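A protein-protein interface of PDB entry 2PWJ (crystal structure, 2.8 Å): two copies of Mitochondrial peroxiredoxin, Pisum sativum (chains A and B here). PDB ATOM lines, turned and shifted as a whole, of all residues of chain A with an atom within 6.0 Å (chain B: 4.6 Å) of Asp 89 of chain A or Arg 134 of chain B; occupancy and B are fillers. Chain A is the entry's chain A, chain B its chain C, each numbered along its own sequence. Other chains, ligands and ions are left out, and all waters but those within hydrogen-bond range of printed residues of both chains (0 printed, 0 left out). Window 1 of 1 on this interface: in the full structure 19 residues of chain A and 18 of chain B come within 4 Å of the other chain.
Hydrophobic or aromatic side chains of chain A within 4 Å of the printed part of chain B: Pro 90, Tyr 91 and Phe 112.
Among the printed residues, Asp or Glu carboxylates within 4 Å of a Lys or Arg side-chain nitrogen of the other chain: Asp 89 of chain A with Arg 134 of chain B (3.1 Å).
Asp 89 of chain A touches just these residues of chain B: Leu 130, Leu 131 and Arg 134.
Of the printed residues of chain B, Pro 90 of chain A touches Leu 130.
Of the printed residues of chain B, Tyr 91 of chain A touches Leu 130 and Leu 131.
Pro 52 of chain B touches none of the printed residues of chain A.
Arg 134 of chain B touches one residue of chain A.
The nearest printed residue of chain A that does not touch Gly 132 of chain B is Asp 89 of chain A (5.6 Å).
CB of Asp 89 of chain A touches O of Leu 130 of chain B, 3.6 Å away.
Leu 131 of chain B touches Asp 89 of chain A.
Pro 90 of chain A touches Leu 130 of chain B.
Tyr 91 of chain A touches Leu 130 of chain B (OH to CD1, 3.4 Å).
CD2 of Tyr 91 of chain A touches CD2 of Leu 131 of chain B (3.4 Å).
Phe 112 of chain A touches Leu 130 of chain B.
Leu 131 of chain B touches Phe 112 of chain A (C to CD2, 3.6 Å).
Phe 112 of chain A touches Gly 132 of chain B (CD2 to N, 3.5 Å).
Positions printed for both chains: 87 and 88.
The side-chain carboxylate of Asp 89 of chain A sits at hydrogen-bond distance from the backbone NH of Thr 92 of chain A.
O of Pro 52 of chain B sits close to NH1 of Arg 134 of chain B (3.3 Å).
The side-chain amide oxygen (OD1) of Asn 88 of chain B is in hydrogen-bond range of the guanidinium group (NH1) of Arg 134 of chain B.
The backbone NH of Tyr 91 of chain A sits at hydrogen-bond distance from the side-chain carboxylate of Asp 89 of chain A (2.9 Å).
The backbone carbonyl oxygen (O) of Arg 134 of chain B is in hydrogen-bond range of the backbone NH (N) of Thr 124 of chain B.
N of Phe 112 of chain A sits close to NE1 of Trp 24 of chain A (2.6 Å).
OD1 of Asp 89 of chain A lies within salt-bridge range of NH2 of Arg 134 of chain B, at 3.1 Å.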
ATOM      1  N   TRP A  24      16.382   9.200 -34.793  1.00  0.00           N
ATOM      2  CA  TRP A  24      15.380  10.132 -35.400  1.00  0.00           C
ATOM      3  C   TRP A  24      15.779  11.505 -36.015  1.00  0.00           C
ATOM      4  O   TRP A  24      16.722  11.478 -36.773  1.00  0.00           O
ATOM      5  CB  TRP A  24      14.203  10.276 -34.417  1.00  0.00           C
ATOM      6  CG  TRP A  24      14.415   9.420 -33.226  1.00  0.00           C
ATOM      7  CD1 TRP A  24      14.888   9.825 -32.017  1.00  0.00           C
ATOM      8  CD2 TRP A  24      14.369   7.989 -33.181  1.00  0.00           C
ATOM      9  NE1 TRP A  24      15.158   8.740 -31.225  1.00  0.00           N
ATOM     10  CE2 TRP A  24      14.849   7.599 -31.915  1.00  0.00           C
ATOM     11  CE3 TRP A  24      13.976   6.999 -34.086  1.00  0.00           C
ATOM     12  CZ2 TRP A  24      14.949   6.252 -31.526  1.00  0.00           C
ATOM     13  CZ3 TRP A  24      14.071   5.645 -33.699  1.00  0.00           C
ATOM     14  CH2 TRP A  24      14.555   5.292 -32.427  1.00  0.00           C
ATOM     15  N   ALA A  86      21.663  12.590 -29.678  1.00  0.00           N
ATOM     16  CA  ALA A  86      21.355  12.848 -28.271  1.00  0.00           C
ATOM     17  C   ALA A  86      20.076  12.167 -27.847  1.00  0.00           C
ATOM     18  O   ALA A  86      19.158  12.028 -28.641  1.00  0.00           O
ATOM     19  CB  ALA A  86      21.231  14.339 -28.033  1.00  0.00           C
ATOM     20  N   ILE A  87      20.018  11.734 -26.595  1.00  0.00           N
ATOM     21  CA  ILE A  87      18.814  11.092 -26.092  1.00  0.00           C
ATOM     22  C   ILE A  87      17.785  12.181 -25.786  1.00  0.00           C
ATOM     23  O   ILE A  87      17.618  12.617 -24.651  1.00  0.00           O
ATOM     24  CB  ILE A  87      19.120  10.246 -24.842  1.00  0.00           C
ATOM     25  CG1 ILE A  87      20.078   9.104 -25.236  1.00  0.00           C
ATOM     26  CG2 ILE A  87      17.834   9.699 -24.253  1.00  0.00           C
ATOM     27  CD1 ILE A  87      20.585   8.242 -24.085  1.00  0.00           C
ATOM     28  N   ASN A  88      17.120  12.621 -26.846  1.00  0.00           N
ATOM     29  CA  ASN A  88      16.090  13.650 -26.814  1.00  0.00           C
ATOM     30  C   ASN A  88      15.126  13.242 -27.921  1.00  0.00           C
ATOM     31  O   ASN A  88      15.539  12.566 -28.873  1.00  0.00           O
ATOM     32  CB  ASN A  88      16.682  15.013 -27.183  1.00  0.00           C
ATOM     33  CG  ASN A  88      17.296  15.730 -26.005  1.00  0.00           C
ATOM     34  OD1 ASN A  88      16.618  16.021 -25.021  1.00  0.00           O
ATOM     35  ND2 ASN A  88      18.586  16.034 -26.100  1.00  0.00           N
ATOM     36  N   ASP A  89      13.856  13.634 -27.820  1.00  0.00           N
ATOM     37  CA  ASP A  89      12.932  13.282 -28.896  1.00  0.00           C
ATOM     38  C   ASP A  89      13.437  14.100 -30.080  1.00  0.00           C
ATOM     39  O   ASP A  89      14.107  15.117 -29.893  1.00  0.00           O
ATOM     40  CB  ASP A  89      11.480  13.643 -28.549  1.00  0.00           C
ATOM     41  CG  ASP A  89      11.280  15.123 -28.292  1.00  0.00           C
ATOM     42  OD1 ASP A  89      11.244  15.523 -27.102  1.00  0.00           O
ATOM     43  OD2 ASP A  89      11.156  15.887 -29.283  1.00  0.00           O
ATOM     44  N   PRO A  90      13.148  13.663 -31.309  1.00  0.00           N
ATOM     45  CA  PRO A  90      13.606  14.389 -32.496  1.00  0.00           C
ATOM     46  C   PRO A  90      13.097  15.809 -32.670  1.00  0.00           C
ATOM     47  O   PRO A  90      13.714  16.602 -33.377  1.00  0.00           O
ATOM     48  CB  PRO A  90      13.176  13.477 -33.644  1.00  0.00           C
ATOM     49  CG  PRO A  90      11.964  12.802 -33.097  1.00  0.00           C
ATOM     50  CD  PRO A  90      12.387  12.463 -31.691  1.00  0.00           C
ATOM     51  N   TYR A  91      11.982  16.134 -32.024  1.00  0.00           N
ATOM     52  CA  TYR A  91      11.390  17.467 -32.145  1.00  0.00           C
ATOM     53  C   TYR A  91      12.127  18.493 -31.299  1.00  0.00           C
ATOM     54  O   TYR A  91      12.207  19.666 -31.676  1.00  0.00           O
ATOM     55  CB  TYR A  91       9.917  17.406 -31.750  1.00  0.00           C
ATOM     56  CG  TYR A  91       9.251  16.174 -32.308  1.00  0.00           C
ATOM     57  CD1 TYR A  91       9.022  16.049 -33.673  1.00  0.00           C
ATOM     58  CD2 TYR A  91       8.959  15.085 -31.489  1.00  0.00           C
ATOM     59  CE1 TYR A  91       8.532  14.868 -34.213  1.00  0.00           C
ATOM     60  CE2 TYR A  91       8.466  13.898 -32.022  1.00  0.00           C
ATOM     61  CZ  TYR A  91       8.257  13.794 -33.383  1.00  0.00           C
ATOM     62  OH  TYR A  91       7.792  12.615 -33.919  1.00  0.00           O
ATOM     63  N   THR A  92      12.663  18.060 -30.158  1.00  0.00           N
ATOM     64  CA  THR A  92      13.421  18.955 -29.292  1.00  0.00           C
ATOM     65  C   THR A  92      14.830  19.122 -29.861  1.00  0.00           C
ATOM     66  O   THR A  92      15.400  20.207 -29.811  1.00  0.00           O
ATOM     67  CB  THR A  92      13.536  18.398 -27.876  1.00  0.00           C
ATOM     68  OG1 THR A  92      12.231  18.247 -27.316  1.00  0.00           O
ATOM     69  CG2 THR A  92      14.334  19.339 -27.004  1.00  0.00           C
ATOM     70  N   VAL A  93      15.388  18.040 -30.401  1.00  0.00           N
ATOM     71  CA  VAL A  93      16.725  18.090 -30.984  1.00  0.00           C
ATOM     72  C   VAL A  93      16.700  19.124 -32.094  1.00  0.00           C
ATOM     73  O   VAL A  93      17.632  19.909 -32.259  1.00  0.00           O
ATOM     74  CB  VAL A  93      17.132  16.723 -31.578  1.00  0.00           C
ATOM     75  CG1 VAL A  93      18.525  16.801 -32.200  1.00  0.00           C
ATOM     76  CG2 VAL A  93      17.099  15.669 -30.492  1.00  0.00           C
ATOM     77  N   ASN A  94      15.604  19.127 -32.843  1.00  0.00           N
ATOM     78  CA  ASN A  94      15.438  20.052 -33.950  1.00  0.00           C
ATOM     79  C   ASN A  94      15.242  21.488 -33.484  1.00  0.00           C
ATOM     80  O   ASN A  94      15.876  22.416 -33.999  1.00  0.00           O
ATOM     81  CB  ASN A  94      14.262  19.616 -34.809  1.00  0.00           C
ATOM     82  CG  ASN A  94      14.065  20.511 -36.011  1.00  0.00           C
ATOM     83  OD1 ASN A  94      13.202  21.387 -36.006  1.00  0.00           O
ATOM     84  ND2 ASN A  94      14.881  20.310 -37.045  1.00  0.00           N
ATOM     85  N   GLY A 110      17.975  12.016 -33.150  1.00  0.00           N
ATOM     86  CA  GLY A 110      17.536  11.815 -31.792  1.00  0.00           C
ATOM     87  C   GLY A 110      17.661  10.333 -31.483  1.00  0.00           C
ATOM     88  O   GLY A 110      17.880   9.523 -32.387  1.00  0.00           O
ATOM     89  N   ASP A 111      17.520   9.977 -30.208  1.00  0.00           N
ATOM     90  CA  ASP A 111      17.588   8.588 -29.747  1.00  0.00           C
ATOM     91  C   ASP A 111      16.709   8.535 -28.497  1.00  0.00           C
ATOM     92  O   ASP A 111      17.192   8.238 -27.402  1.00  0.00           O
ATOM     93  CB  ASP A 111      19.040   8.211 -29.411  1.00  0.00           C
ATOM     94  CG  ASP A 111      19.178   6.780 -28.902  1.00  0.00           C
ATOM     95  OD1 ASP A 111      18.366   5.927 -29.314  1.00  0.00           O
ATOM     96  OD2 ASP A 111      20.104   6.501 -28.110  1.00  0.00           O
ATOM     97  N   PHE A 112      15.419   8.826 -28.668  1.00  0.00           N
ATOM     98  CA  PHE A 112      14.496   8.872 -27.538  1.00  0.00           C
ATOM     99  C   PHE A 112      14.493   7.605 -26.693  1.00  0.00           C
ATOM    100  O   PHE A 112      14.314   7.677 -25.479  1.00  0.00           O
ATOM    101  CB  PHE A 112      13.078   9.236 -28.013  1.00  0.00           C
ATOM    102  CG  PHE A 112      12.273   8.080 -28.516  1.00  0.00           C
ATOM    103  CD1 PHE A 112      12.570   7.483 -29.727  1.00  0.00           C
ATOM    104  CD2 PHE A 112      11.216   7.577 -27.765  1.00  0.00           C
ATOM    105  CE1 PHE A 112      11.838   6.405 -30.191  1.00  0.00           C
ATOM    106  CE2 PHE A 112      10.475   6.496 -28.221  1.00  0.00           C
ATOM    107  CZ  PHE A 112      10.794   5.910 -29.440  1.00  0.00           C
ATOM    108  N   PRO B  52       1.626  16.377 -23.755  1.00  0.00           N
ATOM    109  CA  PRO B  52       2.654  15.447 -24.233  1.00  0.00           C
ATOM    110  C   PRO B  52       4.077  15.958 -24.115  1.00  0.00           C
ATOM    111  O   PRO B  52       4.978  15.204 -23.764  1.00  0.00           O
ATOM    112  CB  PRO B  52       2.227  15.183 -25.670  1.00  0.00           C
ATOM    113  CG  PRO B  52       0.747  15.220 -25.559  1.00  0.00           C
ATOM    114  CD  PRO B  52       0.533  16.469 -24.732  1.00  0.00           C
ATOM    115  N   GLY B  53       4.296  17.232 -24.407  1.00  0.00           N
ATOM    116  CA  GLY B  53       5.650  17.737 -24.274  1.00  0.00           C
ATOM    117  C   GLY B  53       6.050  18.895 -25.154  1.00  0.00           C
ATOM    118  O   GLY B  53       5.422  19.161 -26.180  1.00  0.00           O
ATOM    119  N   ILE B  87       6.347  15.961 -19.096  1.00  0.00           N
ATOM    120  CA  ILE B  87       7.470  15.066 -18.879  1.00  0.00           C
ATOM    121  C   ILE B  87       8.573  15.445 -19.871  1.00  0.00           C
ATOM    122  O   ILE B  87       8.724  14.853 -20.943  1.00  0.00           O
ATOM    123  CB  ILE B  87       7.046  13.587 -19.050  1.00  0.00           C
ATOM    124  CG1 ILE B  87       6.010  13.235 -17.973  1.00  0.00           C
ATOM    125  CG2 ILE B  87       8.254  12.678 -18.957  1.00  0.00           C
ATOM    126  CD1 ILE B  87       5.372  11.865 -18.123  1.00  0.00           C
ATOM    127  N   ASN B  88       9.319  16.473 -19.484  1.00  0.00           N
ATOM    128  CA  ASN B  88      10.441  17.018 -20.242  1.00  0.00           C
ATOM    129  C   ASN B  88      11.413  17.501 -19.172  1.00  0.00           C
ATOM    130  O   ASN B  88      10.993  17.809 -18.052  1.00  0.00           O
ATOM    131  CB  ASN B  88       9.998  18.234 -21.068  1.00  0.00           C
ATOM    132  CG  ASN B  88       9.392  17.856 -22.392  1.00  0.00           C
ATOM    133  OD1 ASN B  88      10.042  17.232 -23.223  1.00  0.00           O
ATOM    134  ND2 ASN B  88       8.142  18.240 -22.605  1.00  0.00           N
ATOM    135  N   LEU B 122      -1.296   9.208 -15.067  1.00  0.00           N
ATOM    136  CA  LEU B 122      -1.547  10.052 -16.218  1.00  0.00           C
ATOM    137  C   LEU B 122      -0.460   9.948 -17.271  1.00  0.00           C
ATOM    138  O   LEU B 122      -0.183  10.905 -17.978  1.00  0.00           O
ATOM    139  CB  LEU B 122      -1.712  11.514 -15.778  1.00  0.00           C
ATOM    140  CG  LEU B 122      -2.967  11.848 -14.965  1.00  0.00           C
ATOM    141  CD1 LEU B 122      -3.061  13.342 -14.732  1.00  0.00           C
ATOM    142  CD2 LEU B 122      -4.178  11.376 -15.733  1.00  0.00           C
ATOM    143  N   THR B 123       0.172   8.786 -17.372  1.00  0.00           N
ATOM    144  CA  THR B 123       1.206   8.574 -18.380  1.00  0.00           C
ATOM    145  C   THR B 123       0.620   7.703 -19.485  1.00  0.00           C
ATOM    146  O   THR B 123      -0.204   6.825 -19.230  1.00  0.00           O
ATOM    147  CB  THR B 123       2.427   7.837 -17.811  1.00  0.00           C
ATOM    148  OG1 THR B 123       2.046   6.507 -17.444  1.00  0.00           O
ATOM    149  CG2 THR B 123       2.970   8.558 -16.599  1.00  0.00           C
ATOM    150  N   THR B 124       1.042   7.949 -20.715  1.00  0.00           N
ATOM    151  CA  THR B 124       0.571   7.166 -21.849  1.00  0.00           C
ATOM    152  C   THR B 124       1.785   6.927 -22.745  1.00  0.00           C
ATOM    153  O   THR B 124       2.708   7.740 -22.775  1.00  0.00           O
ATOM    154  CB  THR B 124      -0.536   7.919 -22.616  1.00  0.00           C
ATOM    155  OG1 THR B 124      -0.954   7.145 -23.743  1.00  0.00           O
ATOM    156  CG2 THR B 124      -0.040   9.280 -23.079  1.00  0.00           C
ATOM    157  N   LEU B 126       3.715   7.117 -25.962  1.00  0.00           N
ATOM    158  CA  LEU B 126       3.714   7.815 -27.240  1.00  0.00           C
ATOM    159  C   LEU B 126       4.955   7.498 -28.043  1.00  0.00           C
ATOM    160  O   LEU B 126       5.509   8.374 -28.707  1.00  0.00           O
ATOM    161  CB  LEU B 126       3.624   9.325 -27.026  1.00  0.00           C
ATOM    162  CG  LEU B 126       2.385   9.756 -26.244  1.00  0.00           C
ATOM    163  CD1 LEU B 126       2.293  11.268 -26.189  1.00  0.00           C
ATOM    164  CD2 LEU B 126       1.145   9.170 -26.910  1.00  0.00           C
ATOM    165  N   LEU B 130       7.365   8.916 -31.541  1.00  0.00           N
ATOM    166  CA  LEU B 130       8.786   9.180 -31.298  1.00  0.00           C
ATOM    167  C   LEU B 130       9.088   9.968 -30.007  1.00  0.00           C
ATOM    168  O   LEU B 130      10.169  10.526 -29.844  1.00  0.00           O
ATOM    169  CB  LEU B 130       9.405   9.890 -32.512  1.00  0.00           C
ATOM    170  CG  LEU B 130       9.179   9.172 -33.846  1.00  0.00           C
ATOM    171  CD1 LEU B 130       9.737  10.011 -34.982  1.00  0.00           C
ATOM    172  CD2 LEU B 130       9.824   7.799 -33.810  1.00  0.00           C
ATOM    173  N   LEU B 131       8.116  10.024 -29.106  1.00  0.00           N
ATOM    174  CA  LEU B 131       8.287  10.666 -27.811  1.00  0.00           C
ATOM    175  C   LEU B 131       8.221   9.444 -26.908  1.00  0.00           C
ATOM    176  O   LEU B 131       7.504   8.490 -27.202  1.00  0.00           O
ATOM    177  CB  LEU B 131       7.118  11.595 -27.501  1.00  0.00           C
ATOM    178  CG  LEU B 131       6.768  12.707 -28.497  1.00  0.00           C
ATOM    179  CD1 LEU B 131       5.462  13.363 -28.081  1.00  0.00           C
ATOM    180  CD2 LEU B 131       7.879  13.738 -28.547  1.00  0.00           C
ATOM    181  N   GLY B 132       8.959   9.426 -25.819  1.00  0.00           N
ATOM    182  CA  GLY B 132       8.878   8.239 -24.985  1.00  0.00           C
ATOM    183  C   GLY B 132       7.541   8.118 -24.274  1.00  0.00           C
ATOM    184  O   GLY B 132       6.495   8.453 -24.814  1.00  0.00           O
ATOM    185  N   ILE B 133       7.581   7.603 -23.056  1.00  0.00           N
ATOM    186  CA  ILE B 133       6.395   7.488 -22.236  1.00  0.00           C
ATOM    187  C   ILE B 133       6.152   8.924 -21.787  1.00  0.00           C
ATOM    188  O   ILE B 133       7.021   9.539 -21.174  1.00  0.00           O
ATOM    189  CB  ILE B 133       6.682   6.608 -21.002  1.00  0.00           C
ATOM    190  CG1 ILE B 133       7.026   5.194 -21.452  1.00  0.00           C
ATOM    191  CG2 ILE B 133       5.512   6.600 -20.063  1.00  0.00           C
ATOM    192  CD1 ILE B 133       6.008   4.576 -22.363  1.00  0.00           C
ATOM    193  N   ARG B 134       4.986   9.473 -22.098  1.00  0.00           N
ATOM    194  CA  ARG B 134       4.688  10.849 -21.713  1.00  0.00           C
ATOM    195  C   ARG B 134       3.383  10.950 -20.931  1.00  0.00           C
ATOM    196  O   ARG B 134       2.750   9.941 -20.617  1.00  0.00           O
ATOM    197  CB  ARG B 134       4.606  11.712 -22.964  1.00  0.00           C
ATOM    198  CG  ARG B 134       5.876  11.713 -23.786  1.00  0.00           C
ATOM    199  CD  ARG B 134       6.894  12.683 -23.185  1.00  0.00           C
ATOM    200  NE  ARG B 134       8.104  12.742 -23.963  1.00  0.00           N
ATOM    201  CZ  ARG B 134       8.607  13.728 -24.702  1.00  0.00           C
ATOM    202  NH1 ARG B 134       8.045  14.919 -24.849  1.00  0.00           N
ATOM    203  NH2 ARG B 134       9.729  13.457 -25.345  1.00  0.00           N
ATOM    204  N   SER B 135       2.980  12.172 -20.615  1.00  0.00           N
ATOM    205  CA  SER B 135       1.742  12.373 -19.888  1.00  0.00           C
ATOM    206  C   SER B 135       0.622  12.569 -20.896  1.00  0.00           C
ATOM    207  O   SER B 135       0.870  12.899 -22.062  1.00  0.00           O
ATOM    208  CB  SER B 135       1.817  13.628 -19.026  1.00  0.00           C
ATOM    209  OG  SER B 135       1.386  14.765 -19.766  1.00  0.00           O
ATOM    210  N   GLU B 136      -0.611  12.372 -20.445  1.00  0.00           N
ATOM    211  CA  GLU B 136      -1.752  12.576 -21.318  1.00  0.00           C
ATOM    212  C   GLU B 136      -2.000  14.072 -21.303  1.00  0.00           C
ATOM    213  O   GLU B 136      -1.338  14.806 -20.570  1.00  0.00           O
ATOM    214  CB  GLU B 136      -2.986  11.865 -20.777  1.00  0.00           C
ATOM    215  CG  GLU B 136      -2.764  10.424 -20.454  1.00  0.00           C
ATOM    216  CD  GLU B 136      -4.009   9.620 -20.672  1.00  0.00           C
ATOM    217  OE1 GLU B 136      -4.447   9.544 -21.837  1.00  0.00           O
ATOM    218  OE2 GLU B 136      -4.552   9.071 -19.689  1.00  0.00           O
